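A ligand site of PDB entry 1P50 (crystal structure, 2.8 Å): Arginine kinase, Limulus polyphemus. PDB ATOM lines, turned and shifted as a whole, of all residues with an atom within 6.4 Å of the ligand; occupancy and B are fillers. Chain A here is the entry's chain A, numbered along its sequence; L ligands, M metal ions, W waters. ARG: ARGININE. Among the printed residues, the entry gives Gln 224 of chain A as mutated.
Residues that only touch the ligand: Ser 62 (3.6 Å), Phe 193 (3.6 Å), Asn 273 (3.8 Å) and His 314 (3.7 Å).
Hydrophobic or aromatic side chains within 4 Å of the ligand: Val 64, Tyr 67, Phe 193 and His 314.
The nearest printed residue that does not touch the ligand is Arg 308 (4.5 Å).
ND2 of Asn 273 is in hydrogen-bond range of OE1 of Gln 224, 3.3 Å away.
OE1 of Gln 224 lies close to NH2 of Arg 228 (3.4 Å).
OG1 of Thr 272 is in hydrogen-bond range of SG of Cys 270 (2.8 Å).
The backbone carbonyl oxygen (O) of Phe 193 lies within hydrogen-bond range of the side-chain hydroxyl (OG) of Ser 55 (2.7 Å).
The backbone NH of Phe 193 is in hydrogen-bond range of the side-chain carboxylate of Asp 191, at 2.7 Å.
The side-chain amide nitrogen (ND2) of Asn 273 sits close to the guanidinium group (NH2) of Arg 228, at 3.4 Å.
The guanidinium group (NH2) of Arg 125 lies within hydrogen-bond range of the side-chain amide oxygen (OD1) of Asn 273, at 2.9 Å.
A nitrogen (NE) of the ligand lies within salt-bridge range of the side-chain carboxylate of Glu 313 (2.6 Å).
O of the ligand is in hydrogen-bond range of N of Val 64.
An oxygen (O) of the ligand lies within hydrogen-bond range of the backbone NH of Gly 63 (2.8 Å).
The side-chain amide oxygen (OE1) of Gln 224 sits at hydrogen-bond distance from a nitrogen (NH1) of the ligand, at 2.9 Å.
A nitrogen (N) of the ligand lies within hydrogen-bond range of the side-chain hydroxyl (OH) of Tyr 67.
SG of Cys 270 lies within hydrogen-bond range of NH1 of the ligand (3.1 Å).
The backbone NH (N) of Gly 65 sits at hydrogen-bond distance from an oxygen (O) of the ligand (3.2 Å).
The side-chain hydroxyl of Thr 272 lies within hydrogen-bond range of a nitrogen (NH1) of the ligand, at 3.3 Å.
Water W2 lies within hydrogen-bond range of OG of Ser 62 (2.7 Å), N of the ligand (2.7 Å) and OG of Ser 55 (3.0 Å).
Water W1 lies within hydrogen-bond range of the side-chain carboxylate of Asp 191 and the side-chain carboxylate of Glu 313.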
ATOM      1  N   SER A  24     -34.342  -3.816  15.038  1.00  0.00           N
ATOM      2  CA  SER A  24     -34.397  -3.311  13.664  1.00  0.00           C
ATOM      3  C   SER A  24     -35.562  -2.328  13.527  1.00  0.00           C
ATOM      4  O   SER A  24     -36.556  -2.417  14.238  1.00  0.00           O
ATOM      5  CB  SER A  24     -34.617  -4.445  12.675  1.00  0.00           C
ATOM      6  OG  SER A  24     -36.001  -4.790  12.583  1.00  0.00           O
ATOM      7  N   SER A  55     -35.734  -9.865   4.119  1.00  0.00           N
ATOM      8  CA  SER A  55     -34.411  -9.851   4.732  1.00  0.00           C
ATOM      9  C   SER A  55     -34.526  -9.485   6.211  1.00  0.00           C
ATOM     10  O   SER A  55     -33.761  -9.973   7.059  1.00  0.00           O
ATOM     11  CB  SER A  55     -33.495  -8.867   4.017  1.00  0.00           C
ATOM     12  OG  SER A  55     -32.193  -8.888   4.569  1.00  0.00           O
ATOM     13  N   ASP A  61     -31.350  -9.601  13.290  1.00  0.00           N
ATOM     14  CA  ASP A  61     -30.287  -8.731  13.759  1.00  0.00           C
ATOM     15  C   ASP A  61     -30.086  -7.534  12.843  1.00  0.00           C
ATOM     16  O   ASP A  61     -29.129  -6.772  12.992  1.00  0.00           O
ATOM     17  CB  ASP A  61     -28.987  -9.528  13.918  1.00  0.00           C
ATOM     18  CG  ASP A  61     -28.477 -10.069  12.601  1.00  0.00           C
ATOM     19  OD1 ASP A  61     -29.299 -10.419  11.718  1.00  0.00           O
ATOM     20  OD2 ASP A  61     -27.246 -10.158  12.454  1.00  0.00           O
ATOM     21  N   SER A  62     -30.983  -7.382  11.880  1.00  0.00           N
ATOM     22  CA  SER A  62     -30.949  -6.266  10.935  1.00  0.00           C
ATOM     23  C   SER A  62     -31.110  -4.951  11.705  1.00  0.00           C
ATOM     24  O   SER A  62     -31.653  -4.933  12.813  1.00  0.00           O
ATOM     25  CB  SER A  62     -32.099  -6.375   9.915  1.00  0.00           C
ATOM     26  OG  SER A  62     -31.988  -7.513   9.069  1.00  0.00           O
ATOM     27  N   GLY A  63     -30.643  -3.855  11.121  1.00  0.00           N
ATOM     28  CA  GLY A  63     -30.774  -2.572  11.763  1.00  0.00           C
ATOM     29  C   GLY A  63     -31.969  -1.882  11.150  1.00  0.00           C
ATOM     30  O   GLY A  63     -32.797  -1.292  11.826  1.00  0.00           O
ATOM     31  N   VAL A  64     -32.054  -1.973   9.829  1.00  0.00           N
ATOM     32  CA  VAL A  64     -33.154  -1.384   9.080  1.00  0.00           C
ATOM     33  C   VAL A  64     -34.140  -2.489   8.741  1.00  0.00           C
ATOM     34  O   VAL A  64     -35.285  -2.443   9.170  1.00  0.00           O
ATOM     35  CB  VAL A  64     -32.647  -0.737   7.797  1.00  0.00           C
ATOM     36  CG1 VAL A  64     -33.823  -0.221   6.992  1.00  0.00           C
ATOM     37  CG2 VAL A  64     -31.686   0.386   8.141  1.00  0.00           C
ATOM     38  N   GLY A  65     -33.682  -3.481   7.970  1.00  0.00           N
ATOM     39  CA  GLY A  65     -34.530  -4.608   7.636  1.00  0.00           C
ATOM     40  C   GLY A  65     -35.312  -4.653   6.326  1.00  0.00           C
ATOM     41  O   GLY A  65     -35.784  -5.727   5.941  1.00  0.00           O
ATOM     42  N   ILE A  66     -35.453  -3.539   5.632  1.00  0.00           N
ATOM     43  CA  ILE A  66     -36.222  -3.539   4.391  1.00  0.00           C
ATOM     44  C   ILE A  66     -35.483  -3.023   3.152  1.00  0.00           C
ATOM     45  O   ILE A  66     -34.458  -2.368   3.232  1.00  0.00           O
ATOM     46  CB  ILE A  66     -37.507  -2.706   4.570  1.00  0.00           C
ATOM     47  CG1 ILE A  66     -37.156  -1.220   4.665  1.00  0.00           C
ATOM     48  CG2 ILE A  66     -38.204  -3.133   5.850  1.00  0.00           C
ATOM     49  CD1 ILE A  66     -38.345  -0.313   4.739  1.00  0.00           C
ATOM     50  N   TYR A  67     -36.034  -3.355   1.987  1.00  0.00           N
ATOM     51  CA  TYR A  67     -35.467  -2.930   0.712  1.00  0.00           C
ATOM     52  C   TYR A  67     -36.591  -2.622  -0.251  1.00  0.00           C
ATOM     53  O   TYR A  67     -37.729  -3.024  -0.028  1.00  0.00           O
ATOM     54  CB  TYR A  67     -34.587  -4.021   0.116  1.00  0.00           C
ATOM     55  CG  TYR A  67     -33.302  -4.279   0.864  1.00  0.00           C
ATOM     56  CD1 TYR A  67     -33.257  -5.174   1.927  1.00  0.00           C
ATOM     57  CD2 TYR A  67     -32.123  -3.621   0.501  1.00  0.00           C
ATOM     58  CE1 TYR A  67     -32.070  -5.421   2.609  1.00  0.00           C
ATOM     59  CE2 TYR A  67     -30.926  -3.852   1.177  1.00  0.00           C
ATOM     60  CZ  TYR A  67     -30.904  -4.749   2.230  1.00  0.00           C
ATOM     61  OH  TYR A  67     -29.713  -4.999   2.881  1.00  0.00           O
ATOM     62  N   TYR A  88     -34.566   6.726  10.276  1.00  0.00           N
ATOM     63  CA  TYR A  88     -33.157   6.616   9.917  1.00  0.00           C
ATOM     64  C   TYR A  88     -32.451   7.923   9.557  1.00  0.00           C
ATOM     65  O   TYR A  88     -31.361   8.187  10.049  1.00  0.00           O
ATOM     66  CB  TYR A  88     -32.957   5.637   8.763  1.00  0.00           C
ATOM     67  CG  TYR A  88     -31.491   5.444   8.413  1.00  0.00           C
ATOM     68  CD1 TYR A  88     -30.668   4.648   9.204  1.00  0.00           C
ATOM     69  CD2 TYR A  88     -30.916   6.115   7.333  1.00  0.00           C
ATOM     70  CE1 TYR A  88     -29.308   4.526   8.958  1.00  0.00           C
ATOM     71  CE2 TYR A  88     -29.547   6.006   7.072  1.00  0.00           C
ATOM     72  CZ  TYR A  88     -28.750   5.214   7.894  1.00  0.00           C
ATOM     73  OH  TYR A  88     -27.390   5.099   7.667  1.00  0.00           O
ATOM     74  N   ARG A 125     -18.287   8.080  -0.936  1.00  0.00           N
ATOM     75  CA  ARG A 125     -18.958   7.408  -2.044  1.00  0.00           C
ATOM     76  C   ARG A 125     -20.411   7.773  -2.251  1.00  0.00           C
ATOM     77  O   ARG A 125     -21.085   8.259  -1.337  1.00  0.00           O
ATOM     78  CB  ARG A 125     -18.859   5.881  -1.868  1.00  0.00           C
ATOM     79  CG  ARG A 125     -19.523   5.293  -0.625  1.00  0.00           C
ATOM     80  CD  ARG A 125     -21.028   5.136  -0.751  1.00  0.00           C
ATOM     81  NE  ARG A 125     -21.551   4.200   0.245  1.00  0.00           N
ATOM     82  CZ  ARG A 125     -22.819   4.162   0.645  1.00  0.00           C
ATOM     83  NH1 ARG A 125     -23.212   3.280   1.543  1.00  0.00           N
ATOM     84  NH2 ARG A 125     -23.710   5.023   0.162  1.00  0.00           N
ATOM     85  N   ASP A 191     -23.247 -11.365   1.123  1.00  0.00           N
ATOM     86  CA  ASP A 191     -23.813 -10.667   2.275  1.00  0.00           C
ATOM     87  C   ASP A 191     -25.166 -11.328   2.569  1.00  0.00           C
ATOM     88  O   ASP A 191     -26.019 -11.422   1.686  1.00  0.00           O
ATOM     89  CB  ASP A 191     -23.994  -9.174   1.942  1.00  0.00           C
ATOM     90  CG  ASP A 191     -24.647  -8.390   3.075  1.00  0.00           C
ATOM     91  OD1 ASP A 191     -25.820  -8.656   3.398  1.00  0.00           O
ATOM     92  OD2 ASP A 191     -23.982  -7.496   3.630  1.00  0.00           O
ATOM     93  N   PHE A 193     -27.702 -10.338   4.400  1.00  0.00           N
ATOM     94  CA  PHE A 193     -28.836  -9.409   4.304  1.00  0.00           C
ATOM     95  C   PHE A 193     -29.240  -9.202   2.847  1.00  0.00           C
ATOM     96  O   PHE A 193     -30.425  -9.162   2.531  1.00  0.00           O
ATOM     97  CB  PHE A 193     -28.496  -8.060   4.920  1.00  0.00           C
ATOM     98  CG  PHE A 193     -27.989  -8.137   6.336  1.00  0.00           C
ATOM     99  CD1 PHE A 193     -26.665  -8.491   6.585  1.00  0.00           C
ATOM    100  CD2 PHE A 193     -28.831  -7.857   7.407  1.00  0.00           C
ATOM    101  CE1 PHE A 193     -26.190  -8.579   7.888  1.00  0.00           C
ATOM    102  CE2 PHE A 193     -28.369  -7.945   8.721  1.00  0.00           C
ATOM    103  CZ  PHE A 193     -27.037  -8.307   8.962  1.00  0.00           C
ATOM    104  N   LEU A 194     -28.250  -9.053   1.964  1.00  0.00           N
ATOM    105  CA  LEU A 194     -28.538  -8.856   0.540  1.00  0.00           C
ATOM    106  C   LEU A 194     -29.052 -10.136  -0.120  1.00  0.00           C
ATOM    107  O   LEU A 194     -29.828 -10.099  -1.086  1.00  0.00           O
ATOM    108  CB  LEU A 194     -27.290  -8.365  -0.201  1.00  0.00           C
ATOM    109  CG  LEU A 194     -26.901  -6.908   0.042  1.00  0.00           C
ATOM    110  CD1 LEU A 194     -25.555  -6.602  -0.599  1.00  0.00           C
ATOM    111  CD2 LEU A 194     -27.990  -5.990  -0.521  1.00  0.00           C
ATOM    112  N   GLN A 224     -25.007  -3.855  -4.340  1.00  0.00           N
ATOM    113  CA  GLN A 224     -26.227  -3.364  -3.724  1.00  0.00           C
ATOM    114  C   GLN A 224     -27.005  -2.427  -4.655  1.00  0.00           C
ATOM    115  O   GLN A 224     -28.223  -2.534  -4.797  1.00  0.00           O
ATOM    116  CB  GLN A 224     -25.900  -2.658  -2.416  1.00  0.00           C
ATOM    117  CG  GLN A 224     -27.076  -2.044  -1.730  1.00  0.00           C
ATOM    118  CD  GLN A 224     -26.797  -1.808  -0.266  1.00  0.00           C
ATOM    119  OE1 GLN A 224     -27.505  -1.053   0.388  1.00  0.00           O
ATOM    120  NE2 GLN A 224     -25.784  -2.479   0.260  1.00  0.00           N
ATOM    121  N   ARG A 228     -21.854   2.379  -7.772  1.00  0.00           N
ATOM    122  CA  ARG A 228     -21.306   2.920  -6.526  1.00  0.00           C
ATOM    123  C   ARG A 228     -20.009   3.594  -6.973  1.00  0.00           C
ATOM    124  O   ARG A 228     -18.999   2.929  -7.230  1.00  0.00           O
ATOM    125  CB  ARG A 228     -21.003   1.804  -5.515  1.00  0.00           C
ATOM    126  CG  ARG A 228     -22.226   1.230  -4.787  1.00  0.00           C
ATOM    127  CD  ARG A 228     -22.893   2.249  -3.870  1.00  0.00           C
ATOM    128  NE  ARG A 228     -24.086   1.706  -3.208  1.00  0.00           N
ATOM    129  CZ  ARG A 228     -24.094   1.138  -2.000  1.00  0.00           C
ATOM    130  NH1 ARG A 228     -22.968   1.034  -1.306  1.00  0.00           N
ATOM    131  NH2 ARG A 228     -25.228   0.669  -1.495  1.00  0.00           N
ATOM    132  N   CYS A 270     -31.635   0.323  -1.050  1.00  0.00           N
ATOM    133  CA  CYS A 270     -31.940   0.416   0.377  1.00  0.00           C
ATOM    134  C   CYS A 270     -32.374   1.836   0.752  1.00  0.00           C
ATOM    135  O   CYS A 270     -31.777   2.816   0.303  1.00  0.00           O
ATOM    136  CB  CYS A 270     -30.728   0.018   1.222  1.00  0.00           C
ATOM    137  SG  CYS A 270     -30.949   0.354   2.993  1.00  0.00           S
ATOM    138  N   PRO A 271     -33.415   1.976   1.591  1.00  0.00           N
ATOM    139  CA  PRO A 271     -33.902   3.295   2.005  1.00  0.00           C
ATOM    140  C   PRO A 271     -32.859   4.144   2.706  1.00  0.00           C
ATOM    141  O   PRO A 271     -33.013   5.359   2.820  1.00  0.00           O
ATOM    142  CB  PRO A 271     -35.084   2.975   2.905  1.00  0.00           C
ATOM    143  CG  PRO A 271     -34.769   1.596   3.426  1.00  0.00           C
ATOM    144  CD  PRO A 271     -34.220   0.911   2.216  1.00  0.00           C
ATOM    145  N   THR A 272     -31.780   3.526   3.157  1.00  0.00           N
ATOM    146  CA  THR A 272     -30.732   4.260   3.858  1.00  0.00           C
ATOM    147  C   THR A 272     -29.789   5.041   2.952  1.00  0.00           C
ATOM    148  O   THR A 272     -29.109   5.952   3.415  1.00  0.00           O
ATOM    149  CB  THR A 272     -29.887   3.322   4.735  1.00  0.00           C
ATOM    150  OG1 THR A 272     -29.225   2.360   3.893  1.00  0.00           O
ATOM    151  CG2 THR A 272     -30.767   2.600   5.734  1.00  0.00           C
ATOM    152  N   ASN A 273     -29.737   4.692   1.671  1.00  0.00           N
ATOM    153  CA  ASN A 273     -28.843   5.355   0.736  1.00  0.00           C
ATOM    154  C   ASN A 273     -29.510   6.328  -0.243  1.00  0.00           C
ATOM    155  O   ASN A 273     -28.887   6.795  -1.194  1.00  0.00           O
ATOM    156  CB  ASN A 273     -28.050   4.295  -0.050  1.00  0.00           C
ATOM    157  CG  ASN A 273     -27.049   3.533   0.830  1.00  0.00           C
ATOM    158  OD1 ASN A 273     -26.194   4.133   1.480  1.00  0.00           O
ATOM    159  ND2 ASN A 273     -27.155   2.208   0.840  1.00  0.00           N
ATOM    160  N   GLN A 306     -21.937   7.298  12.214  1.00  0.00           N
ATOM    161  CA  GLN A 306     -22.114   5.861  12.396  1.00  0.00           C
ATOM    162  C   GLN A 306     -20.762   5.161  12.507  1.00  0.00           C
ATOM    163  O   GLN A 306     -19.783   5.530  11.851  1.00  0.00           O
ATOM    164  CB  GLN A 306     -22.911   5.293  11.219  1.00  0.00           C
ATOM    165  CG  GLN A 306     -23.165   3.789  11.300  1.00  0.00           C
ATOM    166  CD  GLN A 306     -23.971   3.284  10.111  1.00  0.00           C
ATOM    167  OE1 GLN A 306     -23.492   3.305   8.968  1.00  0.00           O
ATOM    168  NE2 GLN A 306     -25.197   2.841  10.373  1.00  0.00           N
ATOM    169  N   ARG A 308     -18.683   1.626  12.095  1.00  0.00           N
ATOM    170  CA  ARG A 308     -18.634   0.324  11.461  1.00  0.00           C
ATOM    171  C   ARG A 308     -17.289  -0.340  11.719  1.00  0.00           C
ATOM    172  O   ARG A 308     -16.351   0.292  12.205  1.00  0.00           O
ATOM    173  CB  ARG A 308     -18.847   0.438   9.949  1.00  0.00           C
ATOM    174  CG  ARG A 308     -20.234   0.907   9.573  1.00  0.00           C
ATOM    175  CD  ARG A 308     -20.488   0.830   8.080  1.00  0.00           C
ATOM    176  NE  ARG A 308     -21.796   1.396   7.762  1.00  0.00           N
ATOM    177  CZ  ARG A 308     -22.365   1.374   6.566  1.00  0.00           C
ATOM    178  NH1 ARG A 308     -21.741   0.800   5.537  1.00  0.00           N
ATOM    179  NH2 ARG A 308     -23.554   1.907   6.386  1.00  0.00           N
ATOM    180  N   GLU A 313     -19.646  -2.640   7.077  1.00  0.00           N
ATOM    181  CA  GLU A 313     -20.746  -2.763   8.007  1.00  0.00           C
ATOM    182  C   GLU A 313     -20.842  -4.246   8.428  1.00  0.00           C
ATOM    183  O   GLU A 313     -20.359  -5.128   7.722  1.00  0.00           O
ATOM    184  CB  GLU A 313     -22.051  -2.280   7.356  1.00  0.00           C
ATOM    185  CG  GLU A 313     -22.653  -3.247   6.368  1.00  0.00           C
ATOM    186  CD  GLU A 313     -23.942  -2.726   5.745  1.00  0.00           C
ATOM    187  OE1 GLU A 313     -24.770  -2.139   6.476  1.00  0.00           O
ATOM    188  OE2 GLU A 313     -24.151  -2.924   4.521  1.00  0.00           O
ATOM    189  N   HIS A 314     -21.444  -4.480   9.590  1.00  0.00           N
ATOM    190  CA  HIS A 314     -21.633  -5.820  10.131  1.00  0.00           C
ATOM    191  C   HIS A 314     -20.328  -6.605  10.361  1.00  0.00           C
ATOM    192  O   HIS A 314     -20.301  -7.832  10.266  1.00  0.00           O
ATOM    193  CB  HIS A 314     -22.586  -6.615   9.236  1.00  0.00           C
ATOM    194  CG  HIS A 314     -23.940  -6.001   9.126  1.00  0.00           C
ATOM    195  ND1 HIS A 314     -24.391  -5.378   7.984  1.00  0.00           N
ATOM    196  CD2 HIS A 314     -24.936  -5.860  10.039  1.00  0.00           C
ATOM    197  CE1 HIS A 314     -25.592  -4.885   8.193  1.00  0.00           C
ATOM    198  NE2 HIS A 314     -25.956  -5.166   9.430  1.00  0.00           N
HETATM  199  N   ARG L   1     -30.205  -4.488   5.769  1.00  0.00           N
HETATM  200  CA  ARG L   1     -29.032  -4.309   6.622  1.00  0.00           C
HETATM  201  C   ARG L   1     -29.427  -3.978   8.068  1.00  0.00           C
HETATM  202  O   ARG L   1     -30.544  -3.546   8.319  1.00  0.00           O
HETATM  203  CB  ARG L   1     -28.133  -3.198   6.074  1.00  0.00           C
HETATM  204  CG  ARG L   1     -28.777  -1.826   5.991  1.00  0.00           C
HETATM  205  CD  ARG L   1     -27.719  -0.729   5.979  1.00  0.00           C
HETATM  206  NE  ARG L   1     -26.662  -1.007   5.008  1.00  0.00           N
HETATM  207  CZ  ARG L   1     -26.826  -0.948   3.687  1.00  0.00           C
HETATM  208  NH1 ARG L   1     -28.003  -0.623   3.189  1.00  0.00           N
HETATM  209  NH2 ARG L   1     -25.824  -1.248   2.886  1.00  0.00           N
HETATM  210 MG    MG M   1     -22.288  -2.163   1.590  1.00  0.00          MG
HETATM  211  O   HOH W   1     -26.336  -5.395   4.204  1.00  0.00           O
HETATM  212  O   HOH W   2     -31.582  -6.690   6.547  1.00  0.00           O
